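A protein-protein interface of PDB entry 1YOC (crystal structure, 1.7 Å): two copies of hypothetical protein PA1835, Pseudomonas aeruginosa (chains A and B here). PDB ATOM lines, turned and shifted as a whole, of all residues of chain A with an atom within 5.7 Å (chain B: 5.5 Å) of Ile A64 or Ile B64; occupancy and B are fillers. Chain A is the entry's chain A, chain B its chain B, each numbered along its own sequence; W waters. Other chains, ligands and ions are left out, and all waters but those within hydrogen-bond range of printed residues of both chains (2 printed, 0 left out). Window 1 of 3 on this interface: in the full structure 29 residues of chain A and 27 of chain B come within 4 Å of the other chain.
The side-chain hydroxyl of Tyr A97 sits at hydrogen-bond distance from the side-chain sulfur of Cys A67 (3.6 Å).
The backbone carbonyl oxygen (O) of Tyr A28 sits close to the side-chain amide oxygen (OD1) of Asn A68 (3.2 Å).
The side-chain amide oxygen (OD1) of Asn B68 sits close to the backbone carbonyl oxygen (O) of Tyr B28.
The backbone carbonyl oxygen (O) of Ala A63 is in hydrogen-bond range of the side-chain sulfur (SG) of Cys A67 (3.5 Å).
The side-chain sulfur (SG) of Cys B67 sits at hydrogen-bond distance from the backbone carbonyl oxygen (O) of Ala B63 (3.5 Å).
Of the printed residues of chain A, Ile B64 touches Tyr A28, Ile A64, Cys A67, Asn A68, Glu A71 and Met A93.
Printed residues of chain B within 4 Å of Tyr A97: Met B93 (3.9 Å).
Of the printed residues of chain A, Phe B29 touches His A62.
Of the printed residues of chain B, Asn A68 touches Tyr B28 (3.0 Å), His B62 (3.4 Å) and Ile B64 (3.5 Å).
Of the printed residues of chain B, Phe A29 touches His B62.
The nearest printed residue of chain B that does not touch Ile A64 is Cys B67 (4.004 Å).
The nearest residue of chain A that does not touch Ile B64 is Phe A29 (5.3 Å).
The nearest printed residue of chain B that does not touch His A62 is Glu B71 (4.1 Å).
Tyr A28 touches His B62, and with the chains exchanged His A62 touches Tyr B28.
Tyr A28 touches Asn B68, and with the chains exchanged Asn A68 touches Tyr B28.
Cys A67 touches Ile B64, but with the chains exchanged Ile A64 does not touch Cys B67 (4.004 Å).
Met A93 touches Tyr B97, and with the chains exchanged Tyr A97 touches Met B93.
Of the 26 pairs that touch across the chains among the printed residues, 23 have their exchanged pair printed and touching as well.
Among the printed residues, pairs that only touch across the chains: His A62 with Phe B29 (3.2 Å), Phe A29 with His B62 (3.4 Å), Ile A64 with Asn B68 (3.4 Å), Tyr A28 with Ala B65 (3.5 Å), Asn A68 with Ile B64 (3.5 Å), His A62 with Tyr B28 (3.5 Å), Ala A65 with Tyr B28 (3.5 Å), Tyr A28 with His B62 (3.6 Å), Ile A64 with Ile B64 (3.6 Å), Glu A71 with Ala B63 (3.7 Å), Ile A64 with Glu B71 (3.7 Å), Tyr A28 with Ile B64 (3.7 Å), Glu A71 with Ile B64 (3.7 Å), Ala A63 with Glu B71 (3.7 Å), Met A93 with Ile B64 (3.8 Å), Met A93 with Met B93 (3.8 Å), Ile A64 with Tyr B28 (3.8 Å), Tyr A97 with Met B93 (3.9 Å), Cys A67 with Ile B64 (3.9 Å), Met A93 with Tyr B97 (3.9 Å) and Cys A67 with Met B93 (3.9 Å).
OH of Tyr A28 sits at hydrogen-bond distance from OD1 of Asn B68, at 3.1 Å.
A ring nitrogen (NE2) of His B62 is in hydrogen-bond range of the side-chain amide nitrogen of Asn A68, 3.4 Å away.
The side-chain hydroxyl of Tyr B28 lies within hydrogen-bond range of the side-chain hydroxyl of Tyr A28, at 3.4 Å.
The side-chain hydroxyl (OH) of Tyr B28 is in hydrogen-bond range of the side-chain amide oxygen (OD1) of Asn A68 (3.0 Å).
The side-chain amide nitrogen (ND2) of Asn B68 sits at hydrogen-bond distance from a ring nitrogen (NE2) of His A62, 3.2 Å away.
Of the 13 printed residues of chain A, 11 touch a printed residue of chain B.
Hydrophobic or aromatic side chains of chain A within 4 Å of the printed part of chain B: Tyr A28, Phe A29, His A62, Ala A63, Ile A64, Met A93 and Tyr A97.
Hydrophobic or aromatic side chains of chain B within 4 Å of the printed part of chain A: Tyr B28, Phe B29, His B62, Ala B63, Ile B64, Met B93 and Tyr B97.
Among the printed residues, no Asp or Glu carboxylate lies within 4 Å of a Lys or Arg side-chain nitrogen of the other chain.
Water W2 lies within hydrogen-bond range of the side-chain carboxylate (OE1) of Glu A71 (2.6 Å), the side-chain hydroxyl (OH) of Tyr B97 (2.7 Å) and the side-chain sulfur (SD) of Met A93 (3.4 Å).
Water W1 lies within hydrogen-bond range of OH of Tyr A97 (2.7 Å), OE1 of Glu B71 (2.7 Å) and SD of Met B93 (3.3 Å).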
ATOM      1  N   TYR A  28       0.158  19.415 -33.759  1.00  0.00           N
ATOM      2  CA  TYR A  28       0.720  20.518 -32.988  1.00  0.00           C
ATOM      3  C   TYR A  28       1.770  21.279 -33.770  1.00  0.00           C
ATOM      4  O   TYR A  28       1.974  22.460 -33.508  1.00  0.00           O
ATOM      5  CB  TYR A  28       1.280  20.055 -31.640  1.00  0.00           C
ATOM      6  CG  TYR A  28       1.494  21.248 -30.732  1.00  0.00           C
ATOM      7  CD1 TYR A  28       0.428  22.117 -30.447  1.00  0.00           C
ATOM      8  CD2 TYR A  28       2.759  21.536 -30.207  1.00  0.00           C
ATOM      9  CE1 TYR A  28       0.613  23.253 -29.651  1.00  0.00           C
ATOM     10  CE2 TYR A  28       2.957  22.678 -29.405  1.00  0.00           C
ATOM     11  CZ  TYR A  28       1.885  23.522 -29.136  1.00  0.00           C
ATOM     12  OH  TYR A  28       2.089  24.644 -28.360  1.00  0.00           O
ATOM     13  N   PHE A  29       2.416  20.638 -34.746  1.00  0.00           N
ATOM     14  CA  PHE A  29       3.403  21.402 -35.551  1.00  0.00           C
ATOM     15  C   PHE A  29       2.717  22.467 -36.413  1.00  0.00           C
ATOM     16  O   PHE A  29       3.311  23.501 -36.759  1.00  0.00           O
ATOM     17  CB  PHE A  29       4.206  20.494 -36.472  1.00  0.00           C
ATOM     18  CG  PHE A  29       5.205  19.595 -35.764  1.00  0.00           C
ATOM     19  CD1 PHE A  29       6.083  20.109 -34.823  1.00  0.00           C
ATOM     20  CD2 PHE A  29       5.307  18.249 -36.102  1.00  0.00           C
ATOM     21  CE1 PHE A  29       7.059  19.290 -34.232  1.00  0.00           C
ATOM     22  CE2 PHE A  29       6.279  17.417 -35.515  1.00  0.00           C
ATOM     23  CZ  PHE A  29       7.164  17.945 -34.575  1.00  0.00           C
ATOM     24  N   HIS A  62       7.530  33.479 -29.495  1.00  0.00           N
ATOM     25  CA  HIS A  62       7.487  32.646 -28.267  1.00  0.00           C
ATOM     26  C   HIS A  62       8.558  31.529 -28.247  1.00  0.00           C
ATOM     27  O   HIS A  62       8.742  30.803 -29.225  1.00  0.00           O
ATOM     28  CB  HIS A  62       6.075  32.052 -28.148  1.00  0.00           C
ATOM     29  CG  HIS A  62       5.751  31.489 -26.795  1.00  0.00           C
ATOM     30  ND1 HIS A  62       4.770  32.021 -25.968  1.00  0.00           N
ATOM     31  CD2 HIS A  62       6.215  30.383 -26.169  1.00  0.00           C
ATOM     32  CE1 HIS A  62       4.642  31.258 -24.890  1.00  0.00           C
ATOM     33  NE2 HIS A  62       5.513  30.258 -24.984  1.00  0.00           N
ATOM     34  N   ALA A  63       9.265  31.449 -27.114  1.00  0.00           N
ATOM     35  CA  ALA A  63      10.302  30.455 -26.880  1.00  0.00           C
ATOM     36  C   ALA A  63       9.861  29.020 -27.224  1.00  0.00           C
ATOM     37  O   ALA A  63      10.646  28.233 -27.707  1.00  0.00           O
ATOM     38  CB  ALA A  63      10.733  30.499 -25.359  1.00  0.00           C
ATOM     39  N   ILE A  64       8.597  28.699 -26.984  1.00  0.00           N
ATOM     40  CA  ILE A  64       8.154  27.333 -27.196  1.00  0.00           C
ATOM     41  C   ILE A  64       7.824  27.115 -28.670  1.00  0.00           C
ATOM     42  O   ILE A  64       7.837  25.980 -29.143  1.00  0.00           O
ATOM     43  CB  ILE A  64       6.953  26.993 -26.211  1.00  0.00           C
ATOM     44  CG1 ILE A  64       7.419  27.193 -24.736  1.00  0.00           C
ATOM     45  CG2 ILE A  64       6.491  25.519 -26.395  1.00  0.00           C
ATOM     46  CD1 ILE A  64       8.667  26.375 -24.295  1.00  0.00           C
ATOM     47  N   ALA A  65       7.530  28.205 -29.397  1.00  0.00           N
ATOM     48  CA  ALA A  65       7.342  28.075 -30.844  1.00  0.00           C
ATOM     49  C   ALA A  65       8.736  27.693 -31.425  1.00  0.00           C
ATOM     50  O   ALA A  65       8.841  26.901 -32.369  1.00  0.00           O
ATOM     51  CB  ALA A  65       6.892  29.404 -31.436  1.00  0.00           C
ATOM     52  N   LEU A  66       9.809  28.247 -30.845  1.00  0.00           N
ATOM     53  CA  LEU A  66      11.156  27.881 -31.309  1.00  0.00           C
ATOM     54  C   LEU A  66      11.423  26.422 -30.994  1.00  0.00           C
ATOM     55  O   LEU A  66      12.013  25.684 -31.802  1.00  0.00           O
ATOM     56  CB  LEU A  66      12.231  28.758 -30.609  1.00  0.00           C
ATOM     57  CG  LEU A  66      12.045  30.246 -30.830  1.00  0.00           C
ATOM     58  CD1 LEU A  66      13.081  31.031 -29.955  1.00  0.00           C
ATOM     59  CD2 LEU A  66      12.194  30.560 -32.317  1.00  0.00           C
ATOM     60  N   CYS A  67      11.010  25.989 -29.816  1.00  0.00           N
ATOM     61  CA  CYS A  67      11.245  24.593 -29.452  1.00  0.00           C
ATOM     62  C   CYS A  67      10.473  23.653 -30.424  1.00  0.00           C
ATOM     63  O   CYS A  67      10.942  22.545 -30.729  1.00  0.00           O
ATOM     64  CB  CYS A  67      10.745  24.309 -28.018  1.00  0.00           C
ATOM     65  SG  CYS A  67      11.664  25.057 -26.667  1.00  0.00           S
ATOM     66  N   ASN A  68       9.283  24.079 -30.829  1.00  0.00           N
ATOM     67  CA  ASN A  68       8.442  23.282 -31.730  1.00  0.00           C
ATOM     68  C   ASN A  68       9.171  23.123 -33.063  1.00  0.00           C
ATOM     69  O   ASN A  68       9.186  22.031 -33.627  1.00  0.00           O
ATOM     70  CB  ASN A  68       7.103  23.996 -31.944  1.00  0.00           C
ATOM     71  CG  ASN A  68       5.896  23.016 -32.164  1.00  0.00           C
ATOM     72  OD1 ASN A  68       4.763  23.460 -32.401  1.00  0.00           O
ATOM     73  ND2 ASN A  68       6.133  21.734 -32.036  1.00  0.00           N
ATOM     74  N   ALA A  69       9.777  24.211 -33.552  1.00  0.00           N
ATOM     75  CA  ALA A  69      10.522  24.167 -34.830  1.00  0.00           C
ATOM     76  C   ALA A  69      11.717  23.244 -34.667  1.00  0.00           C
ATOM     77  O   ALA A  69      12.044  22.478 -35.575  1.00  0.00           O
ATOM     78  CB  ALA A  69      10.997  25.591 -35.234  1.00  0.00           C
ATOM     79  N   GLU A  71      12.018  20.629 -32.625  1.00  0.00           N
ATOM     80  CA  GLU A  71      11.524  19.256 -32.566  1.00  0.00           C
ATOM     81  C   GLU A  71      11.214  18.740 -33.993  1.00  0.00           C
ATOM     82  O   GLU A  71      11.563  17.594 -34.355  1.00  0.00           O
ATOM     83  CB  GLU A  71      10.242  19.238 -31.719  1.00  0.00           C
ATOM     84  CG  GLU A  71       9.537  17.911 -31.721  1.00  0.00           C
ATOM     85  CD  GLU A  71       9.989  16.976 -30.586  1.00  0.00           C
ATOM     86  OE1 GLU A  71      11.153  17.016 -30.149  1.00  0.00           O
ATOM     87  OE2 GLU A  71       9.148  16.164 -30.150  1.00  0.00           O
ATOM     88  N   MET A  93      15.242  16.745 -23.984  1.00  0.00           N
ATOM     89  CA  MET A  93      15.822  17.861 -24.712  1.00  0.00           C
ATOM     90  C   MET A  93      16.328  18.935 -23.769  1.00  0.00           C
ATOM     91  O   MET A  93      15.740  19.164 -22.712  1.00  0.00           O
ATOM     92  CB  MET A  93      14.729  18.448 -25.618  1.00  0.00           C
ATOM     93  CG  MET A  93      15.023  19.817 -26.220  1.00  0.00           C
ATOM     94  SD  MET A  93      13.633  20.407 -27.276  1.00  0.00           S
ATOM     95  CE  MET A  93      12.311  20.919 -26.108  1.00  0.00           C
ATOM     96  N   TYR A  97      18.144  29.834 -24.417  1.00  0.00           N
ATOM     97  CA  TYR A  97      17.520  30.989 -25.074  1.00  0.00           C
ATOM     98  C   TYR A  97      18.599  32.073 -25.102  1.00  0.00           C
ATOM     99  O   TYR A  97      18.957  32.636 -24.045  1.00  0.00           O
ATOM    100  CB  TYR A  97      16.285  31.421 -24.275  1.00  0.00           C
ATOM    101  CG  TYR A  97      15.288  30.251 -24.170  1.00  0.00           C
ATOM    102  CD1 TYR A  97      14.668  29.762 -25.307  1.00  0.00           C
ATOM    103  CD2 TYR A  97      14.936  29.696 -22.925  1.00  0.00           C
ATOM    104  CE1 TYR A  97      13.703  28.757 -25.239  1.00  0.00           C
ATOM    105  CE2 TYR A  97      13.957  28.682 -22.842  1.00  0.00           C
ATOM    106  CZ  TYR A  97      13.354  28.236 -24.014  1.00  0.00           C
ATOM    107  OH  TYR A  97      12.391  27.279 -23.988  1.00  0.00           O
ATOM    108  N   TYR B  28       0.879  32.636 -28.321  1.00  0.00           N
ATOM    109  CA  TYR B  28       1.229  31.249 -28.520  1.00  0.00           C
ATOM    110  C   TYR B  28       0.723  30.299 -27.432  1.00  0.00           C
ATOM    111  O   TYR B  28       0.576  29.122 -27.697  1.00  0.00           O
ATOM    112  CB  TYR B  28       2.748  31.073 -28.792  1.00  0.00           C
ATOM    113  CG  TYR B  28       3.038  29.737 -29.439  1.00  0.00           C
ATOM    114  CD1 TYR B  28       2.484  29.403 -30.691  1.00  0.00           C
ATOM    115  CD2 TYR B  28       3.827  28.774 -28.773  1.00  0.00           C
ATOM    116  CE1 TYR B  28       2.708  28.128 -31.247  1.00  0.00           C
ATOM    117  CE2 TYR B  28       4.061  27.516 -29.330  1.00  0.00           C
ATOM    118  CZ  TYR B  28       3.500  27.202 -30.542  1.00  0.00           C
ATOM    119  OH  TYR B  28       3.678  25.946 -31.021  1.00  0.00           O
ATOM    120  N   PHE B  29       0.468  30.782 -26.225  1.00  0.00           N
ATOM    121  CA  PHE B  29      -0.065  29.891 -25.197  1.00  0.00           C
ATOM    122  C   PHE B  29      -1.459  29.367 -25.583  1.00  0.00           C
ATOM    123  O   PHE B  29      -1.857  28.267 -25.187  1.00  0.00           O
ATOM    124  CB  PHE B  29      -0.111  30.596 -23.850  1.00  0.00           C
ATOM    125  CG  PHE B  29       1.238  30.686 -23.177  1.00  0.00           C
ATOM    126  CD1 PHE B  29       2.035  29.546 -23.018  1.00  0.00           C
ATOM    127  CD2 PHE B  29       1.693  31.896 -22.662  1.00  0.00           C
ATOM    128  CE1 PHE B  29       3.260  29.623 -22.343  1.00  0.00           C
ATOM    129  CE2 PHE B  29       2.901  31.964 -21.988  1.00  0.00           C
ATOM    130  CZ  PHE B  29       3.682  30.828 -21.825  1.00  0.00           C
ATOM    131  N   HIS B  62       1.349  16.154 -27.817  1.00  0.00           N
ATOM    132  CA  HIS B  62       2.666  16.485 -28.336  1.00  0.00           C
ATOM    133  C   HIS B  62       3.634  16.949 -27.271  1.00  0.00           C
ATOM    134  O   HIS B  62       3.277  17.741 -26.402  1.00  0.00           O
ATOM    135  CB  HIS B  62       2.490  17.566 -29.397  1.00  0.00           C
ATOM    136  CG  HIS B  62       3.679  17.758 -30.266  1.00  0.00           C
ATOM    137  ND1 HIS B  62       3.686  17.429 -31.610  1.00  0.00           N
ATOM    138  CD2 HIS B  62       4.844  18.402 -30.023  1.00  0.00           C
ATOM    139  CE1 HIS B  62       4.794  17.891 -32.166  1.00  0.00           C
ATOM    140  NE2 HIS B  62       5.512  18.489 -31.224  1.00  0.00           N
ATOM    141  N   ALA B  63       4.850  16.428 -27.369  1.00  0.00           N
ATOM    142  CA  ALA B  63       5.932  16.777 -26.435  1.00  0.00           C
ATOM    143  C   ALA B  63       6.062  18.295 -26.246  1.00  0.00           C
ATOM    144  O   ALA B  63       6.299  18.780 -25.108  1.00  0.00           O
ATOM    145  CB  ALA B  63       7.289  16.223 -26.976  1.00  0.00           C
ATOM    146  N   ILE B  64       5.936  19.041 -27.336  1.00  0.00           N
ATOM    147  CA  ILE B  64       6.132  20.486 -27.240  1.00  0.00           C
ATOM    148  C   ILE B  64       4.909  21.187 -26.639  1.00  0.00           C
ATOM    149  O   ILE B  64       5.044  22.275 -26.081  1.00  0.00           O
ATOM    150  CB  ILE B  64       6.615  21.064 -28.608  1.00  0.00           C
ATOM    151  CG1 ILE B  64       7.866  20.266 -29.071  1.00  0.00           C
ATOM    152  CG2 ILE B  64       7.014  22.560 -28.466  1.00  0.00           C
ATOM    153  CD1 ILE B  64       9.114  20.374 -28.051  1.00  0.00           C
ATOM    154  N   ALA B  65       3.720  20.568 -26.764  1.00  0.00           N
ATOM    155  CA  ALA B  65       2.523  21.151 -26.115  1.00  0.00           C
ATOM    156  C   ALA B  65       2.734  21.038 -24.572  1.00  0.00           C
ATOM    157  O   ALA B  65       2.341  21.927 -23.788  1.00  0.00           O
ATOM    158  CB  ALA B  65       1.256  20.373 -26.542  1.00  0.00           C
ATOM    159  N   LEU B  66       3.360  19.949 -24.139  1.00  0.00           N
ATOM    160  CA  LEU B  66       3.658  19.754 -22.725  1.00  0.00           C
ATOM    161  C   LEU B  66       4.681  20.823 -22.309  1.00  0.00           C
ATOM    162  O   LEU B  66       4.609  21.379 -21.192  1.00  0.00           O
ATOM    163  CB  LEU B  66       4.237  18.332 -22.481  1.00  0.00           C
ATOM    164  CG  LEU B  66       3.320  17.173 -22.913  1.00  0.00           C
ATOM    165  CD1 LEU B  66       4.109  15.856 -22.879  1.00  0.00           C
ATOM    166  CD2 LEU B  66       2.099  17.111 -22.014  1.00  0.00           C
ATOM    167  N   CYS B  67       5.665  21.086 -23.161  1.00  0.00           N
ATOM    168  CA  CYS B  67       6.666  22.116 -22.829  1.00  0.00           C
ATOM    169  C   CYS B  67       5.960  23.456 -22.692  1.00  0.00           C
ATOM    170  O   CYS B  67       6.322  24.269 -21.825  1.00  0.00           O
ATOM    171  CB  CYS B  67       7.744  22.252 -23.916  1.00  0.00           C
ATOM    172  SG  CYS B  67       8.878  20.866 -24.017  1.00  0.00           S
ATOM    173  N   ASN B  68       4.991  23.717 -23.579  1.00  0.00           N
ATOM    174  CA  ASN B  68       4.269  24.988 -23.509  1.00  0.00           C
ATOM    175  C   ASN B  68       3.548  25.171 -22.166  1.00  0.00           C
ATOM    176  O   ASN B  68       3.548  26.276 -21.576  1.00  0.00           O
ATOM    177  CB  ASN B  68       3.269  25.065 -24.662  1.00  0.00           C
ATOM    178  CG  ASN B  68       3.102  26.504 -25.220  1.00  0.00           C
ATOM    179  OD1 ASN B  68       2.262  26.727 -26.098  1.00  0.00           O
ATOM    180  ND2 ASN B  68       3.908  27.461 -24.734  1.00  0.00           N
ATOM    181  N   ALA B  69       2.931  24.094 -21.664  1.00  0.00           N
ATOM    182  CA  ALA B  69       2.241  24.164 -20.383  1.00  0.00           C
ATOM    183  C   ALA B  69       3.274  24.457 -19.273  1.00  0.00           C
ATOM    184  O   ALA B  69       3.018  25.211 -18.329  1.00  0.00           O
ATOM    185  CB  ALA B  69       1.531  22.791 -20.070  1.00  0.00           C
ATOM    186  N   GLU B  71       6.185  25.987 -19.560  1.00  0.00           N
ATOM    187  CA  GLU B  71       6.636  27.367 -19.673  1.00  0.00           C
ATOM    188  C   GLU B  71       5.582  28.311 -19.043  1.00  0.00           C
ATOM    189  O   GLU B  71       5.929  29.294 -18.378  1.00  0.00           O
ATOM    190  CB  GLU B  71       6.787  27.716 -21.144  1.00  0.00           C
ATOM    191  CG  GLU B  71       7.109  29.144 -21.379  1.00  0.00           C
ATOM    192  CD  GLU B  71       8.594  29.405 -21.375  1.00  0.00           C
ATOM    193  OE1 GLU B  71       9.363  28.667 -20.679  1.00  0.00           O
ATOM    194  OE2 GLU B  71       8.962  30.387 -22.080  1.00  0.00           O
ATOM    195  N   MET B  93      16.154  25.382 -20.584  1.00  0.00           N
ATOM    196  CA  MET B  93      15.138  24.426 -20.135  1.00  0.00           C
ATOM    197  C   MET B  93      15.601  23.021 -20.478  1.00  0.00           C
ATOM    198  O   MET B  93      16.176  22.795 -21.551  1.00  0.00           O
ATOM    199  CB  MET B  93      13.774  24.671 -20.810  1.00  0.00           C
ATOM    200  CG  MET B  93      12.766  23.525 -20.509  1.00  0.00           C
ATOM    201  SD  MET B  93      11.130  23.810 -21.256  1.00  0.00           S
ATOM    202  CE  MET B  93      11.528  23.622 -23.007  1.00  0.00           C
ATOM    203  N   TYR B  97      10.926  13.061 -21.303  1.00  0.00           N
ATOM    204  CA  TYR B  97       9.638  12.516 -21.679  1.00  0.00           C
ATOM    205  C   TYR B  97       9.498  11.174 -20.998  1.00  0.00           C
ATOM    206  O   TYR B  97      10.167  10.209 -21.363  1.00  0.00           O
ATOM    207  CB  TYR B  97       9.578  12.396 -23.203  1.00  0.00           C
ATOM    208  CG  TYR B  97       9.840  13.743 -23.846  1.00  0.00           C
ATOM    209  CD1 TYR B  97       9.015  14.838 -23.559  1.00  0.00           C
ATOM    210  CD2 TYR B  97      10.904  13.929 -24.756  1.00  0.00           C
ATOM    211  CE1 TYR B  97       9.230  16.101 -24.166  1.00  0.00           C
ATOM    212  CE2 TYR B  97      11.122  15.194 -25.363  1.00  0.00           C
ATOM    213  CZ  TYR B  97      10.280  16.255 -25.065  1.00  0.00           C
ATOM    214  OH  TYR B  97      10.466  17.490 -25.666  1.00  0.00           O
HETATM  215  O   HOH W   1      11.398  27.053 -21.472  1.00  0.00           O
HETATM  216  O   HOH W   2      12.117  17.442 -27.790  1.00  0.00           O
